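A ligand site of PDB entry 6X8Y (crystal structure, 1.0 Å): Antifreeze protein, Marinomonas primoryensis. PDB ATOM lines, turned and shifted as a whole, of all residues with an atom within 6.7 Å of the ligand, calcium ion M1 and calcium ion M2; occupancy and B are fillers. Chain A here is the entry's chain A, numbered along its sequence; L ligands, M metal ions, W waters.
An oxygen (O4) of the ligand lies within hydrogen-bond range of the side-chain amide nitrogen (NE2) of Gln 150, 3.0 Å away. An oxygen (O2) of the ligand lies close to the backbone NH (N) of Asp 153 (2.9 Å). N of Gln 123 sits at hydrogen-bond distance from O4 of the ligand (3.5 Å).
The backbone NH of Gln 150 lies close to the side-chain carboxylate of Asp 105 (2.8 Å). The backbone NH of Asp 104 sits at hydrogen-bond distance from the backbone carbonyl oxygen of Val 155. The side-chain carboxylate of Asp 81 lies close to the side-chain hydroxyl of Thr 80, at 2.7 Å. The side-chain carboxylate (OD2) of Asp 81 lies close to the backbone NH (N) of Leu 22 (3.0 Å). The backbone NH of Gln 123 sits at hydrogen-bond distance from the side-chain carboxylate of Asp 105, 2.9 Å away. The backbone NH (N) of Asp 105 is in hydrogen-bond range of the backbone carbonyl oxygen (O) of Trp 148 (2.9 Å). The side-chain amide nitrogen of Asn 122 lies within hydrogen-bond range of the backbone carbonyl oxygen of Leu 22, 3.0 Å away. OD1 of Asn 122 sits at hydrogen-bond distance from NE1 of Trp 148.
Merely in contact with the ligand: Gly 152 (3.5 Å), Ser 124 (3.7 Å) and Asn 122 (3.8 Å). Nine residues have an atom within 4 Å of the ligand: Asp 104, Asp 105, Asn 122, Gln 123, Ser 124, Gln 150, Gly 151, Gly 152 and Asp 153. The nearest printed residue that does not touch the ligand is Asp 149 (4.5 Å).
The nearest printed residue that does not touch calcium ion M1 is Gly 152 (4.2 Å).
The nearest printed residue that does not touch calcium ion M2 is Thr 80 (4.5 Å).
Calcium ion M1 is bound by the side-chain carboxylate (OD1) of Asp 149 (2.3 Å), the side-chain carboxylate (OD1) of Asp 104 (2.4 Å), the backbone carbonyl oxygen (O) of Asp 153 (2.4 Å), the backbone carbonyl oxygen (O) of Gly 151 (2.4 Å), the side-chain carboxylate (OD2) of Asp 105 (2.4 Å), an oxygen (O3) of the ligand (2.5 Å) and an oxygen (O2) of the ligand (2.5 Å).
Calcium ion M2 is bound by OE1 of Gln 21 (2.3 Å), water W4 (2.3 Å), O of Gln 150 (2.3 Å), water W3 (2.4 Å), water W1 (2.4 Å), OD1 of Asp 81 (2.4 Å) and OD2 of Asp 81 (2.5 Å).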
ATOM      1  N   ASN A  19     -20.255   1.762   7.180  1.00  0.00           N
ATOM      2  CA  ASN A  19     -21.147   2.522   8.053  1.00  0.00           C
ATOM      3  C   ASN A  19     -22.587   2.560   7.584  1.00  0.00           C
ATOM      4  O   ASN A  19     -23.416   3.321   8.110  1.00  0.00           O
ATOM      5  CB  ASN A  19     -20.607   3.930   8.287  1.00  0.00           C
ATOM      6  CG  ASN A  19     -19.220   3.852   8.893  1.00  0.00           C
ATOM      7  OD1 ASN A  19     -18.957   3.035   9.808  1.00  0.00           O
ATOM      8  ND2 ASN A  19     -18.296   4.662   8.412  1.00  0.00           N
ATOM      9  N   SER A  20     -22.891   1.738   6.568  1.00  0.00           N
ATOM     10  CA  SER A  20     -24.246   1.444   6.150  1.00  0.00           C
ATOM     11  C   SER A  20     -24.751   0.187   6.847  1.00  0.00           C
ATOM     12  O   SER A  20     -23.963  -0.589   7.404  1.00  0.00           O
ATOM     13  CB  SER A  20     -24.273   1.274   4.631  1.00  0.00           C
ATOM     14  OG  SER A  20     -23.644   0.063   4.221  1.00  0.00           O
ATOM     15  N   GLN A  21     -26.076  -0.005   6.826  1.00  0.00           N
ATOM     16  CA  GLN A  21     -26.686  -1.161   7.477  1.00  0.00           C
ATOM     17  C   GLN A  21     -26.599  -2.406   6.598  1.00  0.00           C
ATOM     18  O   GLN A  21     -26.957  -2.395   5.416  1.00  0.00           O
ATOM     19  CB  GLN A  21     -28.151  -0.850   7.783  1.00  0.00           C
ATOM     20  CG  GLN A  21     -28.989  -2.043   8.167  1.00  0.00           C
ATOM     21  CD  GLN A  21     -28.635  -2.673   9.519  1.00  0.00           C
ATOM     22  OE1 GLN A  21     -27.643  -2.323  10.160  1.00  0.00           O
ATOM     23  NE2 GLN A  21     -29.486  -3.600   9.978  1.00  0.00           N
ATOM     24  N   LEU A  22     -26.185  -3.493   7.210  1.00  0.00           N
ATOM     25  CA  LEU A  22     -26.228  -4.823   6.589  1.00  0.00           C
ATOM     26  C   LEU A  22     -27.467  -5.558   7.104  1.00  0.00           C
ATOM     27  O   LEU A  22     -27.523  -5.920   8.286  1.00  0.00           O
ATOM     28  CB  LEU A  22     -24.950  -5.593   6.923  1.00  0.00           C
ATOM     29  CG  LEU A  22     -23.650  -4.977   6.379  1.00  0.00           C
ATOM     30  CD1 LEU A  22     -22.454  -5.761   6.898  1.00  0.00           C
ATOM     31  CD2 LEU A  22     -23.645  -4.876   4.857  1.00  0.00           C
ATOM     32  N   GLY A  51     -18.473 -12.343  20.766  1.00  0.00           N
ATOM     33  CA  GLY A  51     -18.145 -11.086  21.430  1.00  0.00           C
ATOM     34  C   GLY A  51     -19.301 -10.117  21.320  1.00  0.00           C
ATOM     35  O   GLY A  51     -20.365 -10.428  20.765  1.00  0.00           O
ATOM     36  N   THR A  80     -19.449   0.694  11.701  1.00  0.00           N
ATOM     37  CA  THR A  80     -20.588   0.216  12.489  1.00  0.00           C
ATOM     38  C   THR A  80     -20.923  -1.256  12.199  1.00  0.00           C
ATOM     39  O   THR A  80     -21.358  -1.973  13.124  1.00  0.00           O
ATOM     40  CB  THR A  80     -21.840   1.086  12.248  1.00  0.00           C
ATOM     41  OG1 THR A  80     -22.299   0.960  10.890  1.00  0.00           O
ATOM     42  CG2 THR A  80     -21.556   2.558  12.510  1.00  0.00           C
ATOM     43  N   ASP A  81     -20.725  -1.687  10.961  1.00  0.00           N
ATOM     44  CA  ASP A  81     -21.142  -2.990  10.481  1.00  0.00           C
ATOM     45  C   ASP A  81     -19.955  -3.617   9.760  1.00  0.00           C
ATOM     46  O   ASP A  81     -19.096  -2.901   9.235  1.00  0.00           O
ATOM     47  CB  ASP A  81     -22.311  -2.843   9.465  1.00  0.00           C
ATOM     48  CG  ASP A  81     -23.626  -2.364  10.061  1.00  0.00           C
ATOM     49  OD1 ASP A  81     -23.634  -1.346  10.793  1.00  0.00           O
ATOM     50  OD2 ASP A  81     -24.690  -2.995   9.792  1.00  0.00           O
ATOM     51  N   ASP A 104     -24.401 -15.047  14.693  1.00  0.00           N
ATOM     52  CA  ASP A 104     -25.016 -13.715  14.849  1.00  0.00           C
ATOM     53  C   ASP A 104     -24.082 -12.839  14.007  1.00  0.00           C
ATOM     54  O   ASP A 104     -22.891 -12.773  14.356  1.00  0.00           O
ATOM     55  CB  ASP A 104     -25.060 -13.312  16.313  1.00  0.00           C
ATOM     56  CG  ASP A 104     -25.436 -11.867  16.541  1.00  0.00           C
ATOM     57  OD1 ASP A 104     -25.382 -11.042  15.588  1.00  0.00           O
ATOM     58  OD2 ASP A 104     -25.793 -11.538  17.741  1.00  0.00           O
ATOM     59  N   ASP A 105     -24.502 -12.278  12.869  1.00  0.00           N
ATOM     60  CA  ASP A 105     -25.857 -12.235  12.285  1.00  0.00           C
ATOM     61  C   ASP A 105     -25.997 -13.400  11.290  1.00  0.00           C
ATOM     62  O   ASP A 105     -25.947 -14.552  11.718  1.00  0.00           O
ATOM     63  CB  ASP A 105     -26.137 -10.839  11.721  1.00  0.00           C
ATOM     64  CG  ASP A 105     -26.442  -9.863  12.828  1.00  0.00           C
ATOM     65  OD1 ASP A 105     -27.602  -9.916  13.330  1.00  0.00           O
ATOM     66  OD2 ASP A 105     -25.551  -9.081  13.270  1.00  0.00           O
ATOM     67  N   ASN A 122     -30.654 -10.774   9.734  1.00  0.00           N
ATOM     68  CA  ASN A 122     -30.024 -10.543  11.011  1.00  0.00           C
ATOM     69  C   ASN A 122     -30.662 -11.416  12.081  1.00  0.00           C
ATOM     70  O   ASN A 122     -31.809 -11.843  11.963  1.00  0.00           O
ATOM     71  CB  ASN A 122     -30.054  -9.068  11.383  1.00  0.00           C
ATOM     72  CG  ASN A 122     -29.138  -8.256  10.517  1.00  0.00           C
ATOM     73  OD1 ASN A 122     -28.056  -8.728  10.179  1.00  0.00           O
ATOM     74  ND2 ASN A 122     -29.539  -7.037  10.173  1.00  0.00           N
ATOM     75  N   GLN A 123     -29.876 -11.726  13.123  1.00  0.00           N
ATOM     76  CA  GLN A 123     -30.362 -12.551  14.227  1.00  0.00           C
ATOM     77  C   GLN A 123     -29.411 -12.472  15.398  1.00  0.00           C
ATOM     78  O   GLN A 123     -28.184 -12.472  15.208  1.00  0.00           O
ATOM     79  CB  GLN A 123     -30.547 -14.044  13.839  1.00  0.00           C
ATOM     80  CG  GLN A 123     -29.305 -14.661  13.277  1.00  0.00           C
ATOM     81  CD  GLN A 123     -29.466 -16.140  12.941  1.00  0.00           C
ATOM     82  OE1 GLN A 123     -30.580 -16.644  12.777  1.00  0.00           O
ATOM     83  NE2 GLN A 123     -28.363 -16.823  12.786  1.00  0.00           N
ATOM     84  N   SER A 124     -29.968 -12.455  16.618  1.00  0.00           N
ATOM     85  CA  SER A 124     -29.143 -12.817  17.761  1.00  0.00           C
ATOM     86  C   SER A 124     -28.754 -14.301  17.659  1.00  0.00           C
ATOM     87  O   SER A 124     -29.328 -15.066  16.881  1.00  0.00           O
ATOM     88  CB  SER A 124     -29.874 -12.510  19.058  1.00  0.00           C
ATOM     89  OG  SER A 124     -31.143 -13.090  19.106  1.00  0.00           O
ATOM     90  N   VAL A 125     -27.771 -14.721  18.469  1.00  0.00           N
ATOM     91  CA  VAL A 125     -27.147 -16.028  18.300  1.00  0.00           C
ATOM     92  C   VAL A 125     -28.182 -17.118  18.152  1.00  0.00           C
ATOM     93  O   VAL A 125     -29.099 -17.279  18.967  1.00  0.00           O
ATOM     94  CB  VAL A 125     -26.158 -16.336  19.428  1.00  0.00           C
ATOM     95  CG1 VAL A 125     -26.815 -16.270  20.790  1.00  0.00           C
ATOM     96  CG2 VAL A 125     -25.506 -17.691  19.206  1.00  0.00           C
ATOM     97  N   TRP A 147     -20.263 -14.066   6.075  1.00  0.00           N
ATOM     98  CA  TRP A 147     -20.870 -13.869   7.390  1.00  0.00           C
ATOM     99  C   TRP A 147     -20.801 -12.372   7.670  1.00  0.00           C
ATOM    100  O   TRP A 147     -19.836 -11.723   7.244  1.00  0.00           O
ATOM    101  CB  TRP A 147     -20.104 -14.658   8.488  1.00  0.00           C
ATOM    102  CG  TRP A 147     -20.447 -14.185   9.878  1.00  0.00           C
ATOM    103  CD1 TRP A 147     -21.492 -14.580  10.653  1.00  0.00           C
ATOM    104  CD2 TRP A 147     -19.800 -13.117  10.600  1.00  0.00           C
ATOM    105  NE1 TRP A 147     -21.522 -13.844  11.818  1.00  0.00           N
ATOM    106  CE2 TRP A 147     -20.507 -12.932  11.801  1.00  0.00           C
ATOM    107  CE3 TRP A 147     -18.706 -12.262  10.323  1.00  0.00           C
ATOM    108  CZ2 TRP A 147     -20.175 -11.940  12.732  1.00  0.00           C
ATOM    109  CZ3 TRP A 147     -18.394 -11.285  11.251  1.00  0.00           C
ATOM    110  CH2 TRP A 147     -19.106 -11.144  12.428  1.00  0.00           C
ATOM    111  N   TRP A 148     -21.789 -11.829   8.386  1.00  0.00           N
ATOM    112  CA  TRP A 148     -21.652 -10.442   8.793  1.00  0.00           C
ATOM    113  C   TRP A 148     -22.284 -10.211  10.160  1.00  0.00           C
ATOM    114  O   TRP A 148     -23.047 -11.037  10.677  1.00  0.00           O
ATOM    115  CB  TRP A 148     -22.305  -9.485   7.736  1.00  0.00           C
ATOM    116  CG  TRP A 148     -23.810  -9.486   7.778  1.00  0.00           C
ATOM    117  CD1 TRP A 148     -24.592  -8.654   8.518  1.00  0.00           C
ATOM    118  CD2 TRP A 148     -24.704 -10.432   7.182  1.00  0.00           C
ATOM    119  NE1 TRP A 148     -25.922  -9.001   8.425  1.00  0.00           N
ATOM    120  CE2 TRP A 148     -26.009 -10.090   7.603  1.00  0.00           C
ATOM    121  CE3 TRP A 148     -24.521 -11.504   6.299  1.00  0.00           C
ATOM    122  CZ2 TRP A 148     -27.133 -10.816   7.211  1.00  0.00           C
ATOM    123  CZ3 TRP A 148     -25.642 -12.216   5.924  1.00  0.00           C
ATOM    124  CH2 TRP A 148     -26.925 -11.882   6.367  1.00  0.00           C
ATOM    125  N   ASP A 149     -21.958  -9.029  10.679  1.00  0.00           N
ATOM    126  CA  ASP A 149     -22.517  -8.454  11.897  1.00  0.00           C
ATOM    127  C   ASP A 149     -23.108  -7.087  11.542  1.00  0.00           C
ATOM    128  O   ASP A 149     -22.400  -6.199  11.044  1.00  0.00           O
ATOM    129  CB  ASP A 149     -21.417  -8.268  12.951  1.00  0.00           C
ATOM    130  CG  ASP A 149     -21.923  -7.588  14.197  1.00  0.00           C
ATOM    131  OD1 ASP A 149     -23.084  -7.844  14.573  1.00  0.00           O
ATOM    132  OD2 ASP A 149     -21.193  -6.739  14.776  1.00  0.00           O
ATOM    133  N   GLN A 150     -24.402  -6.913  11.827  1.00  0.00           N
ATOM    134  CA  GLN A 150     -25.047  -5.591  11.699  1.00  0.00           C
ATOM    135  C   GLN A 150     -24.726  -4.681  12.871  1.00  0.00           C
ATOM    136  O   GLN A 150     -25.064  -3.487  12.832  1.00  0.00           O
ATOM    137  CB  GLN A 150     -26.578  -5.732  11.557  1.00  0.00           C
ATOM    138  CG  GLN A 150     -27.270  -6.194  12.840  1.00  0.00           C
ATOM    139  CD  GLN A 150     -28.679  -5.680  13.037  1.00  0.00           C
ATOM    140  OE1 GLN A 150     -29.037  -4.571  12.633  1.00  0.00           O
ATOM    141  NE2 GLN A 150     -29.501  -6.504  13.708  1.00  0.00           N
ATOM    142  N   GLY A 151     -24.129  -5.226  13.933  1.00  0.00           N
ATOM    143  CA  GLY A 151     -23.906  -4.531  15.178  1.00  0.00           C
ATOM    144  C   GLY A 151     -24.297  -5.381  16.350  1.00  0.00           C
ATOM    145  O   GLY A 151     -25.032  -6.389  16.229  1.00  0.00           O
ATOM    146  N   GLY A 152     -23.810  -4.991  17.516  1.00  0.00           N
ATOM    147  CA  GLY A 152     -24.119  -5.698  18.764  1.00  0.00           C
ATOM    148  C   GLY A 152     -23.228  -6.885  18.984  1.00  0.00           C
ATOM    149  O   GLY A 152     -21.991  -6.763  18.931  1.00  0.00           O
ATOM    150  N   ASP A 153     -23.842  -8.046  19.263  1.00  0.00           N
ATOM    151  CA  ASP A 153     -23.081  -9.252  19.467  1.00  0.00           C
ATOM    152  C   ASP A 153     -22.754  -9.904  18.121  1.00  0.00           C
ATOM    153  O   ASP A 153     -23.295  -9.543  17.071  1.00  0.00           O
ATOM    154  CB  ASP A 153     -23.856 -10.193  20.402  1.00  0.00           C
ATOM    155  CG  ASP A 153     -24.067  -9.596  21.810  1.00  0.00           C
ATOM    156  OD1 ASP A 153     -23.165  -8.863  22.270  1.00  0.00           O
ATOM    157  OD2 ASP A 153     -25.092  -9.909  22.441  1.00  0.00           O
ATOM    158  N   TYR A 154     -21.822 -10.867  18.147  1.00  0.00           N
ATOM    159  CA  TYR A 154     -21.332 -11.510  16.936  1.00  0.00           C
ATOM    160  C   TYR A 154     -20.720 -12.847  17.285  1.00  0.00           C
ATOM    161  O   TYR A 154     -20.013 -12.987  18.288  1.00  0.00           O
ATOM    162  CB  TYR A 154     -20.301 -10.607  16.174  1.00  0.00           C
ATOM    163  CG  TYR A 154     -19.320  -9.901  17.085  1.00  0.00           C
ATOM    164  CD1 TYR A 154     -19.644  -8.665  17.641  1.00  0.00           C
ATOM    165  CD2 TYR A 154     -18.122 -10.497  17.451  1.00  0.00           C
ATOM    166  CE1 TYR A 154     -18.796  -8.046  18.531  1.00  0.00           C
ATOM    167  CE2 TYR A 154     -17.263  -9.884  18.370  1.00  0.00           C
ATOM    168  CZ  TYR A 154     -17.623  -8.667  18.924  1.00  0.00           C
ATOM    169  OH  TYR A 154     -16.778  -8.097  19.872  1.00  0.00           O
ATOM    170  N   VAL A 155     -20.949 -13.838  16.410  1.00  0.00           N
ATOM    171  CA  VAL A 155     -20.361 -15.165  16.552  1.00  0.00           C
ATOM    172  C   VAL A 155     -20.516 -15.855  15.206  1.00  0.00           C
ATOM    173  O   VAL A 155     -21.489 -15.622  14.486  1.00  0.00           O
ATOM    174  CB  VAL A 155     -21.014 -15.987  17.707  1.00  0.00           C
ATOM    175  CG1 VAL A 155     -22.495 -16.287  17.474  1.00  0.00           C
ATOM    176  CG2 VAL A 155     -20.217 -17.269  18.017  1.00  0.00           C
HETATM  177  C1  LIG L   1     -27.817  -7.321  18.187  1.00  0.00           C
HETATM  178  C2  LIG L   1     -27.536  -8.768  17.850  1.00  0.00           C
HETATM  179  C3  LIG L   1     -28.177  -9.142  16.535  1.00  0.00           C
HETATM  180  C4  LIG L   1     -29.643  -8.777  16.518  1.00  0.00           C
HETATM  181  C5  LIG L   1     -29.807  -7.341  16.949  1.00  0.00           C
HETATM  182  O1  LIG L   1     -27.332  -7.019  19.471  1.00  0.00           O
HETATM  183  O2  LIG L   1     -26.132  -9.010  17.839  1.00  0.00           O
HETATM  184  O3  LIG L   1     -27.460  -8.467  15.487  1.00  0.00           O
HETATM  185  O4  LIG L   1     -30.137  -8.969  15.207  1.00  0.00           O
HETATM  186  O5  LIG L   1     -29.242  -7.154  18.227  1.00  0.00           O
HETATM  187 CA    CA M   1     -24.972  -8.713  15.613  1.00  0.00          CA
HETATM  188 CA    CA M   2     -25.906  -1.709  11.558  1.00  0.00          CA
HETATM  189  O   HOH W   1     -27.717  -2.102  13.115  1.00  0.00           O
HETATM  190  O   HOH W   2     -32.912  -9.421  15.407  1.00  0.00           O
HETATM  191  O   HOH W   3     -25.316  -0.324  13.453  1.00  0.00           O
HETATM  192  O   HOH W   4     -26.506   0.324  10.632  1.00  0.00           O
HETATM  193  O   HOH W   5     -27.429  -4.393  19.927  1.00  0.00           O
